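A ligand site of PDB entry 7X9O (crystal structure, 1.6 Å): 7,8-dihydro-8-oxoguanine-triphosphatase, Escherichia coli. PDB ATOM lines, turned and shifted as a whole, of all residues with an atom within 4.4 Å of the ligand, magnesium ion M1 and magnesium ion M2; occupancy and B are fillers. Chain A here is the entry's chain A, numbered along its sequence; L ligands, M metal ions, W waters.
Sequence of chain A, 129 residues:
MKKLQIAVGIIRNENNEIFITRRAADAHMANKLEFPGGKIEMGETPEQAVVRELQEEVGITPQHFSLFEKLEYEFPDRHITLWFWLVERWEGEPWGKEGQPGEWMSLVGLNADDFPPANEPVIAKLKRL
Magnesium ion M2 is bound by water W4 (2.1 Å), water W2 (2.2 Å), water W10 (2.3 Å), the side-chain carboxylate of Glu 57 (2.3 Å) and the side-chain carboxylate of Glu 53 (2.4 Å).
Gly 38 touches magnesium ion M1.
Three residues have an atom within 4 Å of magnesium ion M1: Gly 37, Gly 38 and Glu 57.
The nearest printed residue that does not touch magnesium ion M1 is Glu 53 (4.1 Å).
The backbone NH (N) of Gly 38 lies close to the side-chain carboxylate (OE1) of Glu 53, 3.5 Å away.
O of His 28 sits at hydrogen-bond distance from NE of Arg 23 (2.8 Å).
O of Met 29 lies close to NE of Arg 23.
NH1 of Arg 23 is in salt-bridge range of OE1 of Glu 34, at 2.9 Å.
Magnesium ion M1 is bound by water W4, the backbone carbonyl oxygen of Gly 37, water W7, an oxygen (O3) of the ligand, the side-chain carboxylate of Glu 57 and water W9.
Magnesium ion M1 has six donor atoms within binding distance.
Water W7 lies within hydrogen-bond range of OE1 of Glu 34 (2.8 Å), OE1 of Glu 57 (2.8 Å) and N4 of the ligand (3.0 Å).
Water W2 lies within hydrogen-bond range of OE1 of Glu 56 (2.6 Å) and OE2 of Glu 98 (2.8 Å).
Water W11 lies within hydrogen-bond range of an oxygen (O2) of the ligand (2.4 Å) and the backbone NH of Lys 39 (2.8 Å).
Water W1 bridges O1 of the ligand (2.6 Å) and NH2 of Arg 23 (3.4 Å).
Water W6 lies within hydrogen-bond range of an oxygen (O6) of the ligand (2.8 Å) and the guanidinium group of Arg 78 (2.9 Å).
An oxygen (O7) of the ligand lies within hydrogen-bond range of the backbone NH (N) of Phe 35, at 3.1 Å.
ND1 of His 28 is in hydrogen-bond range of O6 of the ligand, at 2.7 Å.
The guanidinium group (NH2) of Arg 23 lies within salt-bridge range of an oxygen (O1) of the ligand (2.7 Å).
The side-chain amide oxygen of Asn 119 sits at hydrogen-bond distance from a nitrogen (N2) of the ligand.
O of Phe 35 sits at hydrogen-bond distance from N3 of the ligand (2.6 Å).
N4 of the ligand sits at hydrogen-bond distance from OE1 of Glu 34.
Residues that only touch the ligand: Ile 6, Val 8, Gly 38, Phe 75, Ile 80, Leu 82, Pro 116 and Ala 118.
Hydrophobic or aromatic side chains that line the ligand: Ile 6, Val 8, His 28, Phe 35, Phe 75, Ile 80, Leu 82, Pro 116 and Ala 118.
Of the 22 residues printed, 14 come within 4 Å of the ligand.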
ATOM      1  N   ILE A   6       0.292  -6.681 -20.446  1.00  0.00           N
ATOM      2  CA  ILE A   6      -0.905  -7.390 -20.005  1.00  0.00           C
ATOM      3  C   ILE A   6      -1.609  -7.974 -21.227  1.00  0.00           C
ATOM      4  O   ILE A   6      -1.844  -7.263 -22.219  1.00  0.00           O
ATOM      5  CB  ILE A   6      -1.860  -6.440 -19.257  1.00  0.00           C
ATOM      6  CG1 ILE A   6      -1.163  -5.710 -18.097  1.00  0.00           C
ATOM      7  CG2 ILE A   6      -3.105  -7.174 -18.810  1.00  0.00           C
ATOM      8  CD1 ILE A   6      -0.670  -6.597 -16.974  1.00  0.00           C
ATOM      9  N   VAL A   8      -5.199  -9.760 -22.482  1.00  0.00           N
ATOM     10  CA  VAL A   8      -6.575  -9.992 -22.097  1.00  0.00           C
ATOM     11  C   VAL A   8      -7.339 -10.569 -23.271  1.00  0.00           C
ATOM     12  O   VAL A   8      -6.952 -10.425 -24.446  1.00  0.00           O
ATOM     13  CB  VAL A   8      -7.274  -8.698 -21.582  1.00  0.00           C
ATOM     14  CG1 VAL A   8      -6.397  -7.991 -20.546  1.00  0.00           C
ATOM     15  CG2 VAL A   8      -7.617  -7.788 -22.727  1.00  0.00           C
ATOM     16  N   ARG A  23     -13.463  -6.868 -11.250  1.00  0.00           N
ATOM     17  CA  ARG A  23     -12.232  -6.901 -10.482  1.00  0.00           C
ATOM     18  C   ARG A  23     -12.507  -6.746  -8.994  1.00  0.00           C
ATOM     19  O   ARG A  23     -13.465  -6.093  -8.579  1.00  0.00           O
ATOM     20  CB  ARG A  23     -11.297  -5.801 -10.966  1.00  0.00           C
ATOM     21  CG  ARG A  23     -10.890  -6.021 -12.419  1.00  0.00           C
ATOM     22  CD  ARG A  23      -9.923  -4.991 -12.935  1.00  0.00           C
ATOM     23  NE  ARG A  23      -8.672  -4.919 -12.189  1.00  0.00           N
ATOM     24  CZ  ARG A  23      -7.630  -5.731 -12.365  1.00  0.00           C
ATOM     25  NH1 ARG A  23      -7.679  -6.717 -13.247  1.00  0.00           N
ATOM     26  NH2 ARG A  23      -6.543  -5.555 -11.621  1.00  0.00           N
ATOM     27  N   HIS A  28      -5.771  -3.214  -8.209  1.00  0.00           N
ATOM     28  CA  HIS A  28      -5.680  -2.086  -9.112  1.00  0.00           C
ATOM     29  C   HIS A  28      -6.926  -2.058  -9.988  1.00  0.00           C
ATOM     30  O   HIS A  28      -7.432  -3.097 -10.402  1.00  0.00           O
ATOM     31  CB  HIS A  28      -4.415  -2.175  -9.963  1.00  0.00           C
ATOM     32  CG  HIS A  28      -4.195  -0.986 -10.838  1.00  0.00           C
ATOM     33  ND1 HIS A  28      -4.266  -1.045 -12.205  1.00  0.00           N
ATOM     34  CD2 HIS A  28      -3.946   0.317 -10.519  1.00  0.00           C
ATOM     35  CE1 HIS A  28      -4.050   0.160 -12.713  1.00  0.00           C
ATOM     36  NE2 HIS A  28      -3.861   1.003 -11.709  1.00  0.00           N
ATOM     37  N   MET A  29      -7.451  -0.852 -10.275  1.00  0.00           N
ATOM     38  CA  MET A  29      -8.713  -0.732 -10.999  1.00  0.00           C
ATOM     39  C   MET A  29      -9.817  -1.509 -10.287  1.00  0.00           C
ATOM     40  O   MET A  29     -10.554  -2.301 -10.883  1.00  0.00           O
ATOM     41  CB  MET A  29      -8.563  -1.166 -12.463  1.00  0.00           C
ATOM     42  CG  MET A  29      -7.811  -0.161 -13.328  1.00  0.00           C
ATOM     43  SD  MET A  29      -8.678   1.431 -13.408  1.00  0.00           S
ATOM     44  CE  MET A  29      -7.647   2.457 -12.343  1.00  0.00           C
ATOM     45  N   GLU A  34     -13.999  -5.955 -16.599  1.00  0.00           N
ATOM     46  CA  GLU A  34     -12.744  -6.236 -17.283  1.00  0.00           C
ATOM     47  C   GLU A  34     -12.925  -7.387 -18.264  1.00  0.00           C
ATOM     48  O   GLU A  34     -13.786  -8.253 -18.080  1.00  0.00           O
ATOM     49  CB  GLU A  34     -11.633  -6.605 -16.296  1.00  0.00           C
ATOM     50  CG  GLU A  34     -12.071  -7.779 -15.427  1.00  0.00           C
ATOM     51  CD  GLU A  34     -10.945  -8.454 -14.689  1.00  0.00           C
ATOM     52  OE1 GLU A  34      -9.790  -7.979 -14.779  1.00  0.00           O
ATOM     53  OE2 GLU A  34     -11.237  -9.480 -14.012  1.00  0.00           O
ATOM     54  N   PHE A  35     -12.076  -7.409 -19.292  1.00  0.00           N
ATOM     55  CA  PHE A  35     -11.817  -8.643 -20.028  1.00  0.00           C
ATOM     56  C   PHE A  35     -10.866  -9.507 -19.210  1.00  0.00           C
ATOM     57  O   PHE A  35      -9.879  -8.993 -18.680  1.00  0.00           O
ATOM     58  CB  PHE A  35     -11.206  -8.329 -21.397  1.00  0.00           C
ATOM     59  CG  PHE A  35     -12.003  -7.332 -22.201  1.00  0.00           C
ATOM     60  CD1 PHE A  35     -13.301  -7.607 -22.606  1.00  0.00           C
ATOM     61  CD2 PHE A  35     -11.445  -6.105 -22.556  1.00  0.00           C
ATOM     62  CE1 PHE A  35     -14.042  -6.699 -23.353  1.00  0.00           C
ATOM     63  CE2 PHE A  35     -12.169  -5.191 -23.313  1.00  0.00           C
ATOM     64  CZ  PHE A  35     -13.472  -5.479 -23.714  1.00  0.00           C
ATOM     65  N   PRO A  36     -11.124 -10.805 -19.054  1.00  0.00           N
ATOM     66  CA  PRO A  36     -10.185 -11.640 -18.298  1.00  0.00           C
ATOM     67  C   PRO A  36      -8.770 -11.539 -18.885  1.00  0.00           C
ATOM     68  O   PRO A  36      -8.600 -11.477 -20.105  1.00  0.00           O
ATOM     69  CB  PRO A  36     -10.764 -13.054 -18.439  1.00  0.00           C
ATOM     70  CG  PRO A  36     -12.245 -12.797 -18.627  1.00  0.00           C
ATOM     71  CD  PRO A  36     -12.284 -11.587 -19.530  1.00  0.00           C
ATOM     72  N   GLY A  37      -7.778 -11.496 -18.016  1.00  0.00           N
ATOM     73  CA  GLY A  37      -6.398 -11.459 -18.477  1.00  0.00           C
ATOM     74  C   GLY A  37      -5.444 -11.119 -17.343  1.00  0.00           C
ATOM     75  O   GLY A  37      -5.818 -11.080 -16.172  1.00  0.00           O
ATOM     76  N   GLY A  38      -4.186 -10.898 -17.726  1.00  0.00           N
ATOM     77  CA  GLY A  38      -3.183 -10.581 -16.728  1.00  0.00           C
ATOM     78  C   GLY A  38      -1.808 -10.476 -17.338  1.00  0.00           C
ATOM     79  O   GLY A  38      -1.635 -10.392 -18.559  1.00  0.00           O
ATOM     80  N   LYS A  39      -0.802 -10.462 -16.465  1.00  0.00           N
ATOM     81  CA  LYS A  39       0.544 -10.097 -16.876  1.00  0.00           C
ATOM     82  C   LYS A  39       1.213 -11.191 -17.720  1.00  0.00           C
ATOM     83  O   LYS A  39       1.144 -12.376 -17.385  1.00  0.00           O
ATOM     84  CB  LYS A  39       1.411  -9.806 -15.653  1.00  0.00           C
ATOM     85  CG  LYS A  39       2.855  -9.459 -15.996  1.00  0.00           C
ATOM     86  CD  LYS A  39       3.728  -9.466 -14.748  1.00  0.00           C
ATOM     87  CE  LYS A  39       5.203  -9.387 -15.126  1.00  0.00           C
ATOM     88  NZ  LYS A  39       6.086  -9.713 -13.962  1.00  0.00           N
ATOM     89  N   GLU A  53      -3.858 -17.127 -19.062  1.00  0.00           N
ATOM     90  CA  GLU A  53      -4.709 -16.293 -18.216  1.00  0.00           C
ATOM     91  C   GLU A  53      -6.176 -16.692 -18.307  1.00  0.00           C
ATOM     92  O   GLU A  53      -6.878 -16.713 -17.288  1.00  0.00           O
ATOM     93  CB  GLU A  53      -4.527 -14.821 -18.569  1.00  0.00           C
ATOM     94  CG  GLU A  53      -3.190 -14.247 -18.136  1.00  0.00           C
ATOM     95  CD  GLU A  53      -3.111 -14.009 -16.641  1.00  0.00           C
ATOM     96  OE1 GLU A  53      -4.174 -13.916 -15.961  1.00  0.00           O
ATOM     97  OE2 GLU A  53      -1.974 -13.850 -16.129  1.00  0.00           O
ATOM     98  N   GLU A  56      -6.640 -19.897 -16.348  1.00  0.00           N
ATOM     99  CA  GLU A  56      -6.629 -19.657 -14.904  1.00  0.00           C
ATOM    100  C   GLU A  56      -7.895 -18.959 -14.440  1.00  0.00           C
ATOM    101  O   GLU A  56      -8.473 -19.317 -13.410  1.00  0.00           O
ATOM    102  CB  GLU A  56      -5.414 -18.812 -14.520  1.00  0.00           C
ATOM    103  CG  GLU A  56      -4.071 -19.489 -14.703  1.00  0.00           C
ATOM    104  CD  GLU A  56      -2.905 -18.570 -14.393  1.00  0.00           C
ATOM    105  OE1 GLU A  56      -3.142 -17.424 -13.941  1.00  0.00           O
ATOM    106  OE2 GLU A  56      -1.748 -18.988 -14.597  1.00  0.00           O
ATOM    107  N   GLU A  57      -8.307 -17.904 -15.163  1.00  0.00           N
ATOM    108  CA  GLU A  57      -9.333 -17.017 -14.631  1.00  0.00           C
ATOM    109  C   GLU A  57     -10.727 -17.520 -14.911  1.00  0.00           C
ATOM    110  O   GLU A  57     -11.609 -17.368 -14.059  1.00  0.00           O
ATOM    111  CB  GLU A  57      -9.154 -15.593 -15.183  1.00  0.00           C
ATOM    112  CG  GLU A  57      -7.938 -14.902 -14.591  1.00  0.00           C
ATOM    113  CD  GLU A  57      -7.947 -13.401 -14.755  1.00  0.00           C
ATOM    114  OE1 GLU A  57      -8.862 -12.843 -15.402  1.00  0.00           O
ATOM    115  OE2 GLU A  57      -7.001 -12.771 -14.221  1.00  0.00           O
ATOM    116  N   PHE A  75      -1.371   4.901 -16.218  1.00  0.00           N
ATOM    117  CA  PHE A  75      -2.138   5.056 -14.991  1.00  0.00           C
ATOM    118  C   PHE A  75      -1.369   5.948 -14.037  1.00  0.00           C
ATOM    119  O   PHE A  75      -0.184   6.222 -14.245  1.00  0.00           O
ATOM    120  CB  PHE A  75      -2.405   3.686 -14.349  1.00  0.00           C
ATOM    121  CG  PHE A  75      -3.418   2.854 -15.081  1.00  0.00           C
ATOM    122  CD1 PHE A  75      -4.785   3.112 -14.939  1.00  0.00           C
ATOM    123  CD2 PHE A  75      -3.026   1.779 -15.861  1.00  0.00           C
ATOM    124  CE1 PHE A  75      -5.732   2.326 -15.593  1.00  0.00           C
ATOM    125  CE2 PHE A  75      -3.967   0.993 -16.506  1.00  0.00           C
ATOM    126  CZ  PHE A  75      -5.317   1.270 -16.386  1.00  0.00           C
ATOM    127  N   ARG A  78       1.432   3.424 -12.700  1.00  0.00           N
ATOM    128  CA  ARG A  78       2.009   2.337 -13.488  1.00  0.00           C
ATOM    129  C   ARG A  78       1.714   2.573 -14.958  1.00  0.00           C
ATOM    130  O   ARG A  78       0.725   3.214 -15.311  1.00  0.00           O
ATOM    131  CB  ARG A  78       1.479   0.963 -13.037  1.00  0.00           C
ATOM    132  CG  ARG A  78       0.006   0.693 -13.321  1.00  0.00           C
ATOM    133  CD  ARG A  78      -0.443  -0.487 -12.493  1.00  0.00           C
ATOM    134  NE  ARG A  78      -0.526  -0.119 -11.083  1.00  0.00           N
ATOM    135  CZ  ARG A  78      -0.598  -0.978 -10.081  1.00  0.00           C
ATOM    136  NH1 ARG A  78      -0.587  -2.291 -10.302  1.00  0.00           N
ATOM    137  NH2 ARG A  78      -0.673  -0.513  -8.839  1.00  0.00           N
ATOM    138  N   ILE A  80       1.080   0.516 -18.509  1.00  0.00           N
ATOM    139  CA  ILE A  80       0.841  -0.818 -19.034  1.00  0.00           C
ATOM    140  C   ILE A  80       0.632  -0.795 -20.537  1.00  0.00           C
ATOM    141  O   ILE A  80       0.139   0.180 -21.119  1.00  0.00           O
ATOM    142  CB  ILE A  80      -0.335  -1.528 -18.336  1.00  0.00           C
ATOM    143  CG1 ILE A  80      -1.666  -0.926 -18.749  1.00  0.00           C
ATOM    144  CG2 ILE A  80      -0.160  -1.542 -16.823  1.00  0.00           C
ATOM    145  CD1 ILE A  80      -2.824  -1.772 -18.311  1.00  0.00           C
ATOM    146  N   LEU A  82      -1.430  -3.061 -23.166  1.00  0.00           N
ATOM    147  CA  LEU A  82      -2.528  -4.007 -23.178  1.00  0.00           C
ATOM    148  C   LEU A  82      -2.641  -4.657 -24.542  1.00  0.00           C
ATOM    149  O   LEU A  82      -2.721  -3.974 -25.560  1.00  0.00           O
ATOM    150  CB  LEU A  82      -3.843  -3.310 -22.836  1.00  0.00           C
ATOM    151  CG  LEU A  82      -4.036  -3.081 -21.350  1.00  0.00           C
ATOM    152  CD1 LEU A  82      -4.837  -1.829 -21.149  1.00  0.00           C
ATOM    153  CD2 LEU A  82      -4.739  -4.280 -20.729  1.00  0.00           C
ATOM    154  N   GLU A  98     -11.906 -18.250 -10.487  1.00  0.00           N
ATOM    155  CA  GLU A  98     -11.180 -17.710  -9.338  1.00  0.00           C
ATOM    156  C   GLU A  98     -12.128 -17.118  -8.296  1.00  0.00           C
ATOM    157  O   GLU A  98     -11.686 -16.359  -7.437  1.00  0.00           O
ATOM    158  CB  GLU A  98     -10.155 -16.675  -9.796  1.00  0.00           C
ATOM    159  CG  GLU A  98      -8.960 -17.287 -10.544  1.00  0.00           C
ATOM    160  CD  GLU A  98      -7.958 -16.242 -11.034  1.00  0.00           C
ATOM    161  OE1 GLU A  98      -8.299 -15.042 -11.082  1.00  0.00           O
ATOM    162  OE2 GLU A  98      -6.824 -16.637 -11.400  1.00  0.00           O
ATOM    163  N   PRO A 116     -11.769  -0.067 -16.962  1.00  0.00           N
ATOM    164  CA  PRO A 116     -10.637   0.849 -16.853  1.00  0.00           C
ATOM    165  C   PRO A 116     -10.592   1.776 -18.037  1.00  0.00           C
ATOM    166  O   PRO A 116     -10.976   1.399 -19.171  1.00  0.00           O
ATOM    167  CB  PRO A 116      -9.426  -0.092 -16.831  1.00  0.00           C
ATOM    168  CG  PRO A 116      -9.994  -1.403 -16.261  1.00  0.00           C
ATOM    169  CD  PRO A 116     -11.340  -1.484 -16.925  1.00  0.00           C
ATOM    170  N   ALA A 118      -8.299   2.654 -19.890  1.00  0.00           N
ATOM    171  CA  ALA A 118      -7.491   2.118 -20.985  1.00  0.00           C
ATOM    172  C   ALA A 118      -8.344   1.408 -22.025  1.00  0.00           C
ATOM    173  O   ALA A 118      -7.960   1.318 -23.191  1.00  0.00           O
ATOM    174  CB  ALA A 118      -6.445   1.177 -20.404  1.00  0.00           C
ATOM    175  N   ASN A 119      -9.511   0.882 -21.622  1.00  0.00           N
ATOM    176  CA  ASN A 119     -10.337   0.091 -22.527  1.00  0.00           C
ATOM    177  C   ASN A 119     -11.213   0.930 -23.439  1.00  0.00           C
ATOM    178  O   ASN A 119     -11.833   0.363 -24.349  1.00  0.00           O
ATOM    179  CB  ASN A 119     -11.221  -0.868 -21.708  1.00  0.00           C
ATOM    180  CG  ASN A 119     -10.416  -1.931 -20.992  1.00  0.00           C
ATOM    181  OD1 ASN A 119      -9.252  -1.742 -20.660  1.00  0.00           O
ATOM    182  ND2 ASN A 119     -11.060  -3.063 -20.759  1.00  0.00           N
HETATM  183  O1  LIG L   1      -4.720  -7.478 -12.160  1.00  0.00           O
HETATM  184  P1  LIG L   1      -4.292  -8.290 -13.344  1.00  0.00           P
HETATM  185  O2  LIG L   1      -3.214  -9.283 -13.006  1.00  0.00           O
HETATM  186  O3  LIG L   1      -5.451  -8.897 -14.134  1.00  0.00           O
HETATM  187  O4  LIG L   1      -3.531  -7.267 -14.345  1.00  0.00           O
HETATM  188  C1  LIG L   1      -4.260  -6.472 -15.266  1.00  0.00           C
HETATM  189  C2  LIG L   1      -3.772  -5.014 -15.267  1.00  0.00           C
HETATM  190  O5  LIG L   1      -4.244  -4.453 -16.480  1.00  0.00           O
HETATM  191  C3  LIG L   1      -4.390  -4.155 -14.164  1.00  0.00           C
HETATM  192  O6  LIG L   1      -3.514  -3.047 -13.930  1.00  0.00           O
HETATM  193  C4  LIG L   1      -5.642  -3.586 -14.792  1.00  0.00           C
HETATM  194  C5  LIG L   1      -5.195  -3.418 -16.238  1.00  0.00           C
HETATM  195  N1  LIG L   1      -6.344  -3.578 -17.155  1.00  0.00           N
HETATM  196  C6  LIG L   1      -6.913  -2.654 -17.913  1.00  0.00           C
HETATM  197  N2  LIG L   1      -7.950  -3.089 -18.658  1.00  0.00           N
HETATM  198  C7  LIG L   1      -8.018  -4.430 -18.337  1.00  0.00           C
HETATM  199  C8  LIG L   1      -8.845  -5.483 -18.741  1.00  0.00           C
HETATM  200  O7  LIG L   1      -9.799  -5.337 -19.549  1.00  0.00           O
HETATM  201  N3  LIG L   1      -8.615  -6.716 -18.227  1.00  0.00           N
HETATM  202  C9  LIG L   1      -7.642  -6.945 -17.339  1.00  0.00           C
HETATM  203  N4  LIG L   1      -7.427  -8.197 -16.862  1.00  0.00           N
HETATM  204  N5  LIG L   1      -6.828  -5.958 -16.939  1.00  0.00           N
HETATM  205  C10 LIG L   1      -7.006  -4.707 -17.416  1.00  0.00           C
HETATM  206  O8  LIG L   1      -6.511  -1.413 -17.890  1.00  0.00           O
HETATM  207 MG    MG M   1      -6.266 -10.818 -14.212  1.00  0.00          MG
HETATM  208 MG    MG M   2      -4.918 -13.616 -13.676  1.00  0.00          MG
HETATM  209  O   HOH W   1      -6.052  -8.690 -10.295  1.00  0.00           O
HETATM  210  O   HOH W   2      -4.953 -15.727 -13.239  1.00  0.00           O
HETATM  211  O   HOH W   3      -2.847  -5.776 -10.906  1.00  0.00           O
HETATM  212  O   HOH W   4      -4.520 -11.596 -13.552  1.00  0.00           O
HETATM  213  O   HOH W   5      -0.722  -6.797 -13.258  1.00  0.00           O
HETATM  214  O   HOH W   6      -1.322  -4.106 -12.470  1.00  0.00           O
HETATM  215  O   HOH W   7      -8.178 -10.219 -14.772  1.00  0.00           O
HETATM  216  O   HOH W   8      -2.362  -9.666 -10.449  1.00  0.00           O
HETATM  217  O   HOH W   9      -7.079 -10.697 -12.193  1.00  0.00           O
HETATM  218  O   HOH W  10      -5.993 -13.716 -11.700  1.00  0.00           O
HETATM  219  O   HOH W  11      -1.285 -10.538 -13.702  1.00  0.00           O
